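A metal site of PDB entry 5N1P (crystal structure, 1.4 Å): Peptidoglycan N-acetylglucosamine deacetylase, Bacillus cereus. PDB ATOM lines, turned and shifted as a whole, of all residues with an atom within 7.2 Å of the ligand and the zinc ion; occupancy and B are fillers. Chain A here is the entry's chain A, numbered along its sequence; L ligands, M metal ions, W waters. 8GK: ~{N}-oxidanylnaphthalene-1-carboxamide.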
ATOM      1  N   PHE A   8     -11.340  -0.110  11.059  1.00  0.00           N
ATOM      2  CA  PHE A   8     -10.615  -0.503   9.852  1.00  0.00           C
ATOM      3  C   PHE A   8      -9.134  -0.574  10.160  1.00  0.00           C
ATOM      4  O   PHE A   8      -8.539   0.428  10.536  1.00  0.00           O
ATOM      5  CB  PHE A   8     -10.852   0.507   8.717  1.00  0.00           C
ATOM      6  CG  PHE A   8     -12.285   0.617   8.321  1.00  0.00           C
ATOM      7  CD1 PHE A   8     -12.832  -0.292   7.435  1.00  0.00           C
ATOM      8  CD2 PHE A   8     -13.097   1.610   8.869  1.00  0.00           C
ATOM      9  CE1 PHE A   8     -14.177  -0.211   7.063  1.00  0.00           C
ATOM     10  CE2 PHE A   8     -14.444   1.698   8.504  1.00  0.00           C
ATOM     11  CZ  PHE A   8     -14.986   0.775   7.604  1.00  0.00           C
ATOM     12  N   ASP A   9      -8.565  -1.754   9.972  1.00  0.00           N
ATOM     13  CA  ASP A   9      -7.162  -2.043  10.284  1.00  0.00           C
ATOM     14  C   ASP A   9      -6.261  -2.073   9.044  1.00  0.00           C
ATOM     15  O   ASP A   9      -6.713  -2.382   7.940  1.00  0.00           O
ATOM     16  CB  ASP A   9      -7.028  -3.421  10.950  1.00  0.00           C
ATOM     17  CG  ASP A   9      -7.529  -3.464  12.379  1.00  0.00           C
ATOM     18  OD1 ASP A   9      -8.022  -2.450  12.879  1.00  0.00           O
ATOM     19  OD2 ASP A   9      -7.424  -4.562  12.999  1.00  0.00           O
ATOM     20  N   ASP A  10      -4.986  -1.778   9.290  1.00  0.00           N
ATOM     21  CA  ASP A  10      -3.836  -2.091   8.418  1.00  0.00           C
ATOM     22  C   ASP A  10      -3.518  -0.978   7.421  1.00  0.00           C
ATOM     23  O   ASP A  10      -2.560  -1.092   6.647  1.00  0.00           O
ATOM     24  CB  ASP A  10      -3.990  -3.415   7.636  1.00  0.00           C
ATOM     25  CG  ASP A  10      -4.125  -4.651   8.534  1.00  0.00           C
ATOM     26  OD1 ASP A  10      -3.852  -4.593   9.748  1.00  0.00           O
ATOM     27  OD2 ASP A  10      -4.483  -5.727   7.993  1.00  0.00           O
ATOM     28  N   PHE A  33      -7.190   2.011  12.502  1.00  0.00           N
ATOM     29  CA  PHE A  33      -5.994   1.585  13.235  1.00  0.00           C
ATOM     30  C   PHE A  33      -4.867   1.390  12.229  1.00  0.00           C
ATOM     31  O   PHE A  33      -4.926   0.512  11.374  1.00  0.00           O
ATOM     32  CB  PHE A  33      -6.272   0.289  14.024  1.00  0.00           C
ATOM     33  CG  PHE A  33      -7.255   0.493  15.158  1.00  0.00           C
ATOM     34  CD1 PHE A  33      -6.875   1.191  16.299  1.00  0.00           C
ATOM     35  CD2 PHE A  33      -8.526  -0.053  15.087  1.00  0.00           C
ATOM     36  CE1 PHE A  33      -7.747   1.348  17.357  1.00  0.00           C
ATOM     37  CE2 PHE A  33      -9.423   0.120  16.152  1.00  0.00           C
ATOM     38  CZ  PHE A  33      -9.034   0.821  17.280  1.00  0.00           C
ATOM     39  N   ILE A  35      -0.935   1.298  10.480  1.00  0.00           N
ATOM     40  CA  ILE A  35       0.411   0.728  10.557  1.00  0.00           C
ATOM     41  C   ILE A  35       1.434   1.801  10.226  1.00  0.00           C
ATOM     42  O   ILE A  35       1.244   2.550   9.275  1.00  0.00           O
ATOM     43  CB  ILE A  35       0.561  -0.455   9.606  1.00  0.00           C
ATOM     44  CG1 ILE A  35      -0.359  -1.596  10.064  1.00  0.00           C
ATOM     45  CG2 ILE A  35       2.016  -0.893   9.534  1.00  0.00           C
ATOM     46  CD1 ILE A  35      -0.336  -2.815   9.162  1.00  0.00           C
ATOM     47  N   HIS A  59      -1.869   0.576  15.129  1.00  0.00           N
ATOM     48  CA  HIS A  59      -1.916  -0.879  14.853  1.00  0.00           C
ATOM     49  C   HIS A  59      -0.502  -1.464  14.720  1.00  0.00           C
ATOM     50  O   HIS A  59      -0.343  -2.526  14.139  1.00  0.00           O
ATOM     51  CB  HIS A  59      -2.711  -1.145  13.574  1.00  0.00           C
ATOM     52  CG  HIS A  59      -3.141  -2.582  13.389  1.00  0.00           C
ATOM     53  ND1 HIS A  59      -3.633  -3.355  14.422  1.00  0.00           N
ATOM     54  CD2 HIS A  59      -3.203  -3.351  12.278  1.00  0.00           C
ATOM     55  CE1 HIS A  59      -3.964  -4.553  13.952  1.00  0.00           C
ATOM     56  NE2 HIS A  59      -3.713  -4.577  12.657  1.00  0.00           N
ATOM     57  N   HIS A  63       3.693  -5.185  12.692  1.00  0.00           N
ATOM     58  CA  HIS A  63       2.612  -6.178  12.614  1.00  0.00           C
ATOM     59  C   HIS A  63       3.185  -7.600  12.729  1.00  0.00           C
ATOM     60  O   HIS A  63       2.680  -8.536  12.120  1.00  0.00           O
ATOM     61  CB  HIS A  63       1.819  -6.010  11.314  1.00  0.00           C
ATOM     62  CG  HIS A  63       0.404  -6.513  11.382  1.00  0.00           C
ATOM     63  ND1 HIS A  63       0.083  -7.858  11.378  1.00  0.00           N
ATOM     64  CD2 HIS A  63      -0.778  -5.847  11.417  1.00  0.00           C
ATOM     65  CE1 HIS A  63      -1.232  -7.990  11.425  1.00  0.00           C
ATOM     66  NE2 HIS A  63      -1.774  -6.794  11.445  1.00  0.00           N
ATOM     67  N   TYR A  69       4.751  -9.668  20.874  1.00  0.00           N
ATOM     68  CA  TYR A  69       4.273 -10.372  22.055  1.00  0.00           C
ATOM     69  C   TYR A  69       5.375 -11.179  22.738  1.00  0.00           C
ATOM     70  O   TYR A  69       5.673 -10.929  23.902  1.00  0.00           O
ATOM     71  CB  TYR A  69       3.073 -11.241  21.690  1.00  0.00           C
ATOM     72  CG  TYR A  69       2.013 -10.394  21.012  1.00  0.00           C
ATOM     73  CD1 TYR A  69       1.439  -9.309  21.683  1.00  0.00           C
ATOM     74  CD2 TYR A  69       1.591 -10.655  19.713  1.00  0.00           C
ATOM     75  CE1 TYR A  69       0.487  -8.503  21.085  1.00  0.00           C
ATOM     76  CE2 TYR A  69       0.632  -9.858  19.107  1.00  0.00           C
ATOM     77  CZ  TYR A  69       0.090  -8.779  19.793  1.00  0.00           C
ATOM     78  OH  TYR A  69      -0.850  -7.978  19.203  1.00  0.00           O
ATOM     79  N   ARG A  97      -4.983  -1.169  18.658  1.00  0.00           N
ATOM     80  CA  ARG A  97      -5.634  -2.417  18.235  1.00  0.00           C
ATOM     81  C   ARG A  97      -4.523  -3.444  18.016  1.00  0.00           C
ATOM     82  O   ARG A  97      -3.637  -3.237  17.189  1.00  0.00           O
ATOM     83  CB  ARG A  97      -6.454  -2.155  16.968  1.00  0.00           C
ATOM     84  CG  ARG A  97      -6.731  -3.327  16.020  1.00  0.00           C
ATOM     85  CD  ARG A  97      -7.828  -4.275  16.505  1.00  0.00           C
ATOM     86  NE  ARG A  97      -9.102  -3.698  16.927  1.00  0.00           N
ATOM     87  CZ  ARG A  97     -10.105  -3.356  16.119  1.00  0.00           C
ATOM     88  NH1 ARG A  97      -9.964  -3.393  14.803  1.00  0.00           N
ATOM     89  NH2 ARG A  97     -11.256  -2.921  16.643  1.00  0.00           N
ATOM     90  N   PRO A  98      -4.516  -4.525  18.796  1.00  0.00           N
ATOM     91  CA  PRO A  98      -3.409  -5.477  18.661  1.00  0.00           C
ATOM     92  C   PRO A  98      -3.457  -6.253  17.359  1.00  0.00           C
ATOM     93  O   PRO A  98      -4.487  -6.830  17.020  1.00  0.00           O
ATOM     94  CB  PRO A  98      -3.597  -6.456  19.836  1.00  0.00           C
ATOM     95  CG  PRO A  98      -4.579  -5.806  20.751  1.00  0.00           C
ATOM     96  CD  PRO A  98      -5.433  -4.880  19.903  1.00  0.00           C
ATOM     97  N   PRO A  99      -2.338  -6.283  16.625  1.00  0.00           N
ATOM     98  CA  PRO A  99      -2.289  -7.242  15.521  1.00  0.00           C
ATOM     99  C   PRO A  99      -2.571  -8.657  16.046  1.00  0.00           C
ATOM    100  O   PRO A  99      -2.022  -9.058  17.072  1.00  0.00           O
ATOM    101  CB  PRO A  99      -0.854  -7.105  15.018  1.00  0.00           C
ATOM    102  CG  PRO A  99      -0.503  -5.665  15.300  1.00  0.00           C
ATOM    103  CD  PRO A  99      -1.180  -5.367  16.616  1.00  0.00           C
ATOM    104  N   TYR A 100      -3.424  -9.387  15.336  1.00  0.00           N
ATOM    105  CA  TYR A 100      -3.831 -10.759  15.681  1.00  0.00           C
ATOM    106  C   TYR A 100      -4.693 -10.808  16.946  1.00  0.00           C
ATOM    107  O   TYR A 100      -5.005 -11.907  17.448  1.00  0.00           O
ATOM    108  CB  TYR A 100      -2.614 -11.682  15.822  1.00  0.00           C
ATOM    109  CG  TYR A 100      -1.694 -11.556  14.630  1.00  0.00           C
ATOM    110  CD1 TYR A 100      -2.060 -12.083  13.387  1.00  0.00           C
ATOM    111  CD2 TYR A 100      -0.506 -10.857  14.721  1.00  0.00           C
ATOM    112  CE1 TYR A 100      -1.225 -11.933  12.284  1.00  0.00           C
ATOM    113  CE2 TYR A 100       0.315 -10.689  13.626  1.00  0.00           C
ATOM    114  CZ  TYR A 100      -0.049 -11.232  12.411  1.00  0.00           C
ATOM    115  OH  TYR A 100       0.775 -11.042  11.324  1.00  0.00           O
ATOM    116  N   GLY A 101      -5.119  -9.651  17.437  1.00  0.00           N
ATOM    117  CA  GLY A 101      -5.940  -9.605  18.645  1.00  0.00           C
ATOM    118  C   GLY A 101      -5.097  -9.758  19.906  1.00  0.00           C
ATOM    119  O   GLY A 101      -3.956 -10.185  19.842  1.00  0.00           O
ATOM    120  N   TRP A 124     -12.401  -6.626  19.234  1.00  0.00           N
ATOM    121  CA  TRP A 124     -13.630  -6.420  18.478  1.00  0.00           C
ATOM    122  C   TRP A 124     -14.698  -7.360  18.965  1.00  0.00           C
ATOM    123  O   TRP A 124     -14.389  -8.279  19.719  1.00  0.00           O
ATOM    124  CB  TRP A 124     -13.374  -6.615  16.980  1.00  0.00           C
ATOM    125  CG  TRP A 124     -12.714  -7.918  16.681  1.00  0.00           C
ATOM    126  CD1 TRP A 124     -13.348  -9.112  16.418  1.00  0.00           C
ATOM    127  CD2 TRP A 124     -11.313  -8.196  16.645  1.00  0.00           C
ATOM    128  NE1 TRP A 124     -12.424 -10.100  16.208  1.00  0.00           N
ATOM    129  CE2 TRP A 124     -11.163  -9.568  16.341  1.00  0.00           C
ATOM    130  CE3 TRP A 124     -10.164  -7.411  16.840  1.00  0.00           C
ATOM    131  CZ2 TRP A 124      -9.908 -10.181  16.227  1.00  0.00           C
ATOM    132  CZ3 TRP A 124      -8.921  -8.020  16.733  1.00  0.00           C
ATOM    133  CH2 TRP A 124      -8.811  -9.395  16.420  1.00  0.00           C
ATOM    134  N   ASP A 127     -16.291 -10.089  13.855  1.00  0.00           N
ATOM    135  CA  ASP A 127     -15.261 -10.265  12.832  1.00  0.00           C
ATOM    136  C   ASP A 127     -15.942 -10.430  11.471  1.00  0.00           C
ATOM    137  O   ASP A 127     -16.709 -11.370  11.276  1.00  0.00           O
ATOM    138  CB  ASP A 127     -14.387 -11.466  13.180  1.00  0.00           C
ATOM    139  CG  ASP A 127     -13.331 -11.773  12.128  1.00  0.00           C
ATOM    140  OD1 ASP A 127     -13.195 -11.030  11.126  1.00  0.00           O
ATOM    141  OD2 ASP A 127     -12.621 -12.789  12.311  1.00  0.00           O
ATOM    142  N   TRP A 131     -11.146 -11.249   5.122  1.00  0.00           N
ATOM    143  CA  TRP A 131      -9.982 -11.920   4.547  1.00  0.00           C
ATOM    144  C   TRP A 131     -10.328 -13.241   3.841  1.00  0.00           C
ATOM    145  O   TRP A 131      -9.563 -13.709   2.992  1.00  0.00           O
ATOM    146  CB  TRP A 131      -8.936 -12.215   5.637  1.00  0.00           C
ATOM    147  CG  TRP A 131      -9.411 -13.175   6.687  1.00  0.00           C
ATOM    148  CD1 TRP A 131     -10.061 -12.862   7.850  1.00  0.00           C
ATOM    149  CD2 TRP A 131      -9.243 -14.611   6.699  1.00  0.00           C
ATOM    150  NE1 TRP A 131     -10.335 -13.999   8.557  1.00  0.00           N
ATOM    151  CE2 TRP A 131      -9.834 -15.082   7.890  1.00  0.00           C
ATOM    152  CE3 TRP A 131      -8.680 -15.527   5.811  1.00  0.00           C
ATOM    153  CZ2 TRP A 131      -9.863 -16.434   8.218  1.00  0.00           C
ATOM    154  CZ3 TRP A 131      -8.687 -16.880   6.147  1.00  0.00           C
ATOM    155  CH2 TRP A 131      -9.288 -17.318   7.347  1.00  0.00           C
ATOM    156  N   LEU A 161     -14.708  -5.553  13.076  1.00  0.00           N
ATOM    157  CA  LEU A 161     -13.373  -5.650  12.490  1.00  0.00           C
ATOM    158  C   LEU A 161     -13.426  -5.764  10.969  1.00  0.00           C
ATOM    159  O   LEU A 161     -13.967  -6.735  10.420  1.00  0.00           O
ATOM    160  CB  LEU A 161     -12.615  -6.857  13.053  1.00  0.00           C
ATOM    161  CG  LEU A 161     -11.274  -7.153  12.368  1.00  0.00           C
ATOM    162  CD1 LEU A 161     -10.245  -6.036  12.608  1.00  0.00           C
ATOM    163  CD2 LEU A 161     -10.715  -8.515  12.792  1.00  0.00           C
ATOM    164  N   MET A 162     -12.863  -4.758  10.308  1.00  0.00           N
ATOM    165  CA  MET A 162     -12.690  -4.765   8.868  1.00  0.00           C
ATOM    166  C   MET A 162     -11.293  -4.244   8.524  1.00  0.00           C
ATOM    167  O   MET A 162     -10.557  -3.782   9.403  1.00  0.00           O
ATOM    168  CB  MET A 162     -13.758  -3.926   8.168  1.00  0.00           C
ATOM    169  CG  MET A 162     -15.142  -4.441   8.457  1.00  0.00           C
ATOM    170  SD  MET A 162     -16.422  -3.511   7.618  1.00  0.00           S
ATOM    171  CE  MET A 162     -16.161  -4.075   5.939  1.00  0.00           C
ATOM    172  N   HIS A 163     -10.937  -4.322   7.251  1.00  0.00           N
ATOM    173  CA  HIS A 163      -9.618  -3.910   6.790  1.00  0.00           C
ATOM    174  C   HIS A 163      -9.773  -3.069   5.540  1.00  0.00           C
ATOM    175  O   HIS A 163     -10.228  -3.581   4.515  1.00  0.00           O
ATOM    176  CB  HIS A 163      -8.721  -5.137   6.520  1.00  0.00           C
ATOM    177  CG  HIS A 163      -8.531  -6.023   7.711  1.00  0.00           C
ATOM    178  ND1 HIS A 163      -9.453  -6.978   8.090  1.00  0.00           N
ATOM    179  CD2 HIS A 163      -7.532  -6.094   8.623  1.00  0.00           C
ATOM    180  CE1 HIS A 163      -9.033  -7.606   9.166  1.00  0.00           C
ATOM    181  NE2 HIS A 163      -7.867  -7.082   9.521  1.00  0.00           N
ATOM    182  N   ILE A 165      -7.669  -1.977   3.548  1.00  0.00           N
ATOM    183  CA  ILE A 165      -6.650  -2.230   2.533  1.00  0.00           C
ATOM    184  C   ILE A 165      -7.116  -3.257   1.502  1.00  0.00           C
ATOM    185  O   ILE A 165      -6.399  -3.556   0.548  1.00  0.00           O
ATOM    186  CB  ILE A 165      -5.323  -2.696   3.149  1.00  0.00           C
ATOM    187  CG1 ILE A 165      -5.548  -3.938   4.015  1.00  0.00           C
ATOM    188  CG2 ILE A 165      -4.739  -1.559   3.960  1.00  0.00           C
ATOM    189  CD1 ILE A 165      -4.282  -4.724   4.294  1.00  0.00           C
ATOM    190  N   PHE A 200     -10.403  -9.030  24.638  1.00  0.00           N
ATOM    191  CA  PHE A 200     -10.619 -10.459  24.818  1.00  0.00           C
ATOM    192  C   PHE A 200     -10.250 -10.929  26.214  1.00  0.00           C
ATOM    193  O   PHE A 200     -10.715 -11.984  26.649  1.00  0.00           O
ATOM    194  CB  PHE A 200      -9.821 -11.245  23.765  1.00  0.00           C
ATOM    195  CG  PHE A 200     -10.314 -11.049  22.352  1.00  0.00           C
ATOM    196  CD1 PHE A 200     -11.673 -10.977  22.077  1.00  0.00           C
ATOM    197  CD2 PHE A 200      -9.412 -10.929  21.307  1.00  0.00           C
ATOM    198  CE1 PHE A 200     -12.126 -10.799  20.771  1.00  0.00           C
ATOM    199  CE2 PHE A 200      -9.856 -10.748  20.001  1.00  0.00           C
ATOM    200  CZ  PHE A 200     -11.215 -10.676  19.727  1.00  0.00           C
HETATM  201  C1  8GK L   1      -5.520  -8.165  12.708  1.00  0.00           C
HETATM  202  C2  8GK L   1      -5.852  -9.598  12.925  1.00  0.00           C
HETATM  203  C3  8GK L   1      -5.235 -10.540  12.116  1.00  0.00           C
HETATM  204  C4  8GK L   1      -5.502 -11.897  12.313  1.00  0.00           C
HETATM  205  C5  8GK L   1      -6.377 -12.309  13.318  1.00  0.00           C
HETATM  206  C6  8GK L   1      -6.989 -11.350  14.128  1.00  0.00           C
HETATM  207  C7  8GK L   1      -6.717 -10.008  13.931  1.00  0.00           C
HETATM  208  C8  8GK L   1      -4.886 -12.831  11.483  1.00  0.00           C
HETATM  209  C9  8GK L   1      -4.009 -12.426  10.484  1.00  0.00           C
HETATM  210  C10 8GK L   1      -3.751 -11.072  10.287  1.00  0.00           C
HETATM  211  C11 8GK L   1      -4.356 -10.142  11.110  1.00  0.00           C
HETATM  212  O12 8GK L   1      -4.386  -7.813  12.973  1.00  0.00           O
HETATM  213  N13 8GK L   1      -6.409  -7.303  12.202  1.00  0.00           N
HETATM  214  O14 8GK L   1      -5.923  -6.281  11.397  1.00  0.00           O
HETATM  215 ZN    ZN M   1      -3.812  -6.158  11.221  1.00  0.00          ZN
HETATM  216  O   HOH W   1      -4.303  -7.647   9.554  1.00  0.00           O
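A nitrogen (N13) of the ligand lies within hydrogen-bond range of the side-chain carboxylate (OD2) of Asp 9 (3.0 Å).
A ring nitrogen (NE2) of His 163 is in hydrogen-bond range of a nitrogen (N13) of the ligand, at 3.1 Å.
O12 of the ligand sits close to N of Tyr 100 (3.0 Å).
A ring nitrogen (ND1) of His 59 lies within hydrogen-bond range of the backbone carbonyl oxygen (O) of Arg 97 (2.8 Å).
O of His 63 lies within hydrogen-bond range of OH of Tyr 100 (3.2 Å).
The backbone NH (N) of Asp 10 sits at hydrogen-bond distance from the backbone carbonyl oxygen (O) of Phe 33, 3.1 Å away.
The guanidinium group (NH1) of Arg 97 is in salt-bridge range of the side-chain carboxylate (OD1) of Asp 9.
The backbone NH (N) of Asp 9 is in hydrogen-bond range of the backbone carbonyl oxygen (O) of Met 162, at 2.9 Å.
The side-chain hydroxyl of Tyr 69 sits at hydrogen-bond distance from the backbone carbonyl oxygen of Pro 99 (2.7 Å).
Merely in contact with the ligand: Trp 124, Pro 99 and Gly 101.
Within 4 Å of the ligand: Asp 9, Asp 10, His 59, His 63, Pro 99, Tyr 100, Gly 101, Trp 124 and His 163.
The nearest printed residue that does not touch the ligand is Leu 161 (4.1 Å).
Of the 21 residues printed, 3 come within 4 Å of the zinc ion.
The zinc ion is bound by an oxygen (O14) of the ligand (2.1 Å), a ring nitrogen (NE2) of His 59 (2.1 Å), a ring nitrogen (NE2) of His 63 (2.1 Å), the side-chain carboxylate (OD1) of Asp 10 (2.1 Å), water W1 (2.3 Å) and an oxygen (O12) of the ligand (2.5 Å).
The zinc ion has six donor atoms within binding distance.
Water W1 bridges the side-chain carboxylate of Asp 10 and a nitrogen (N13) of the ligand.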
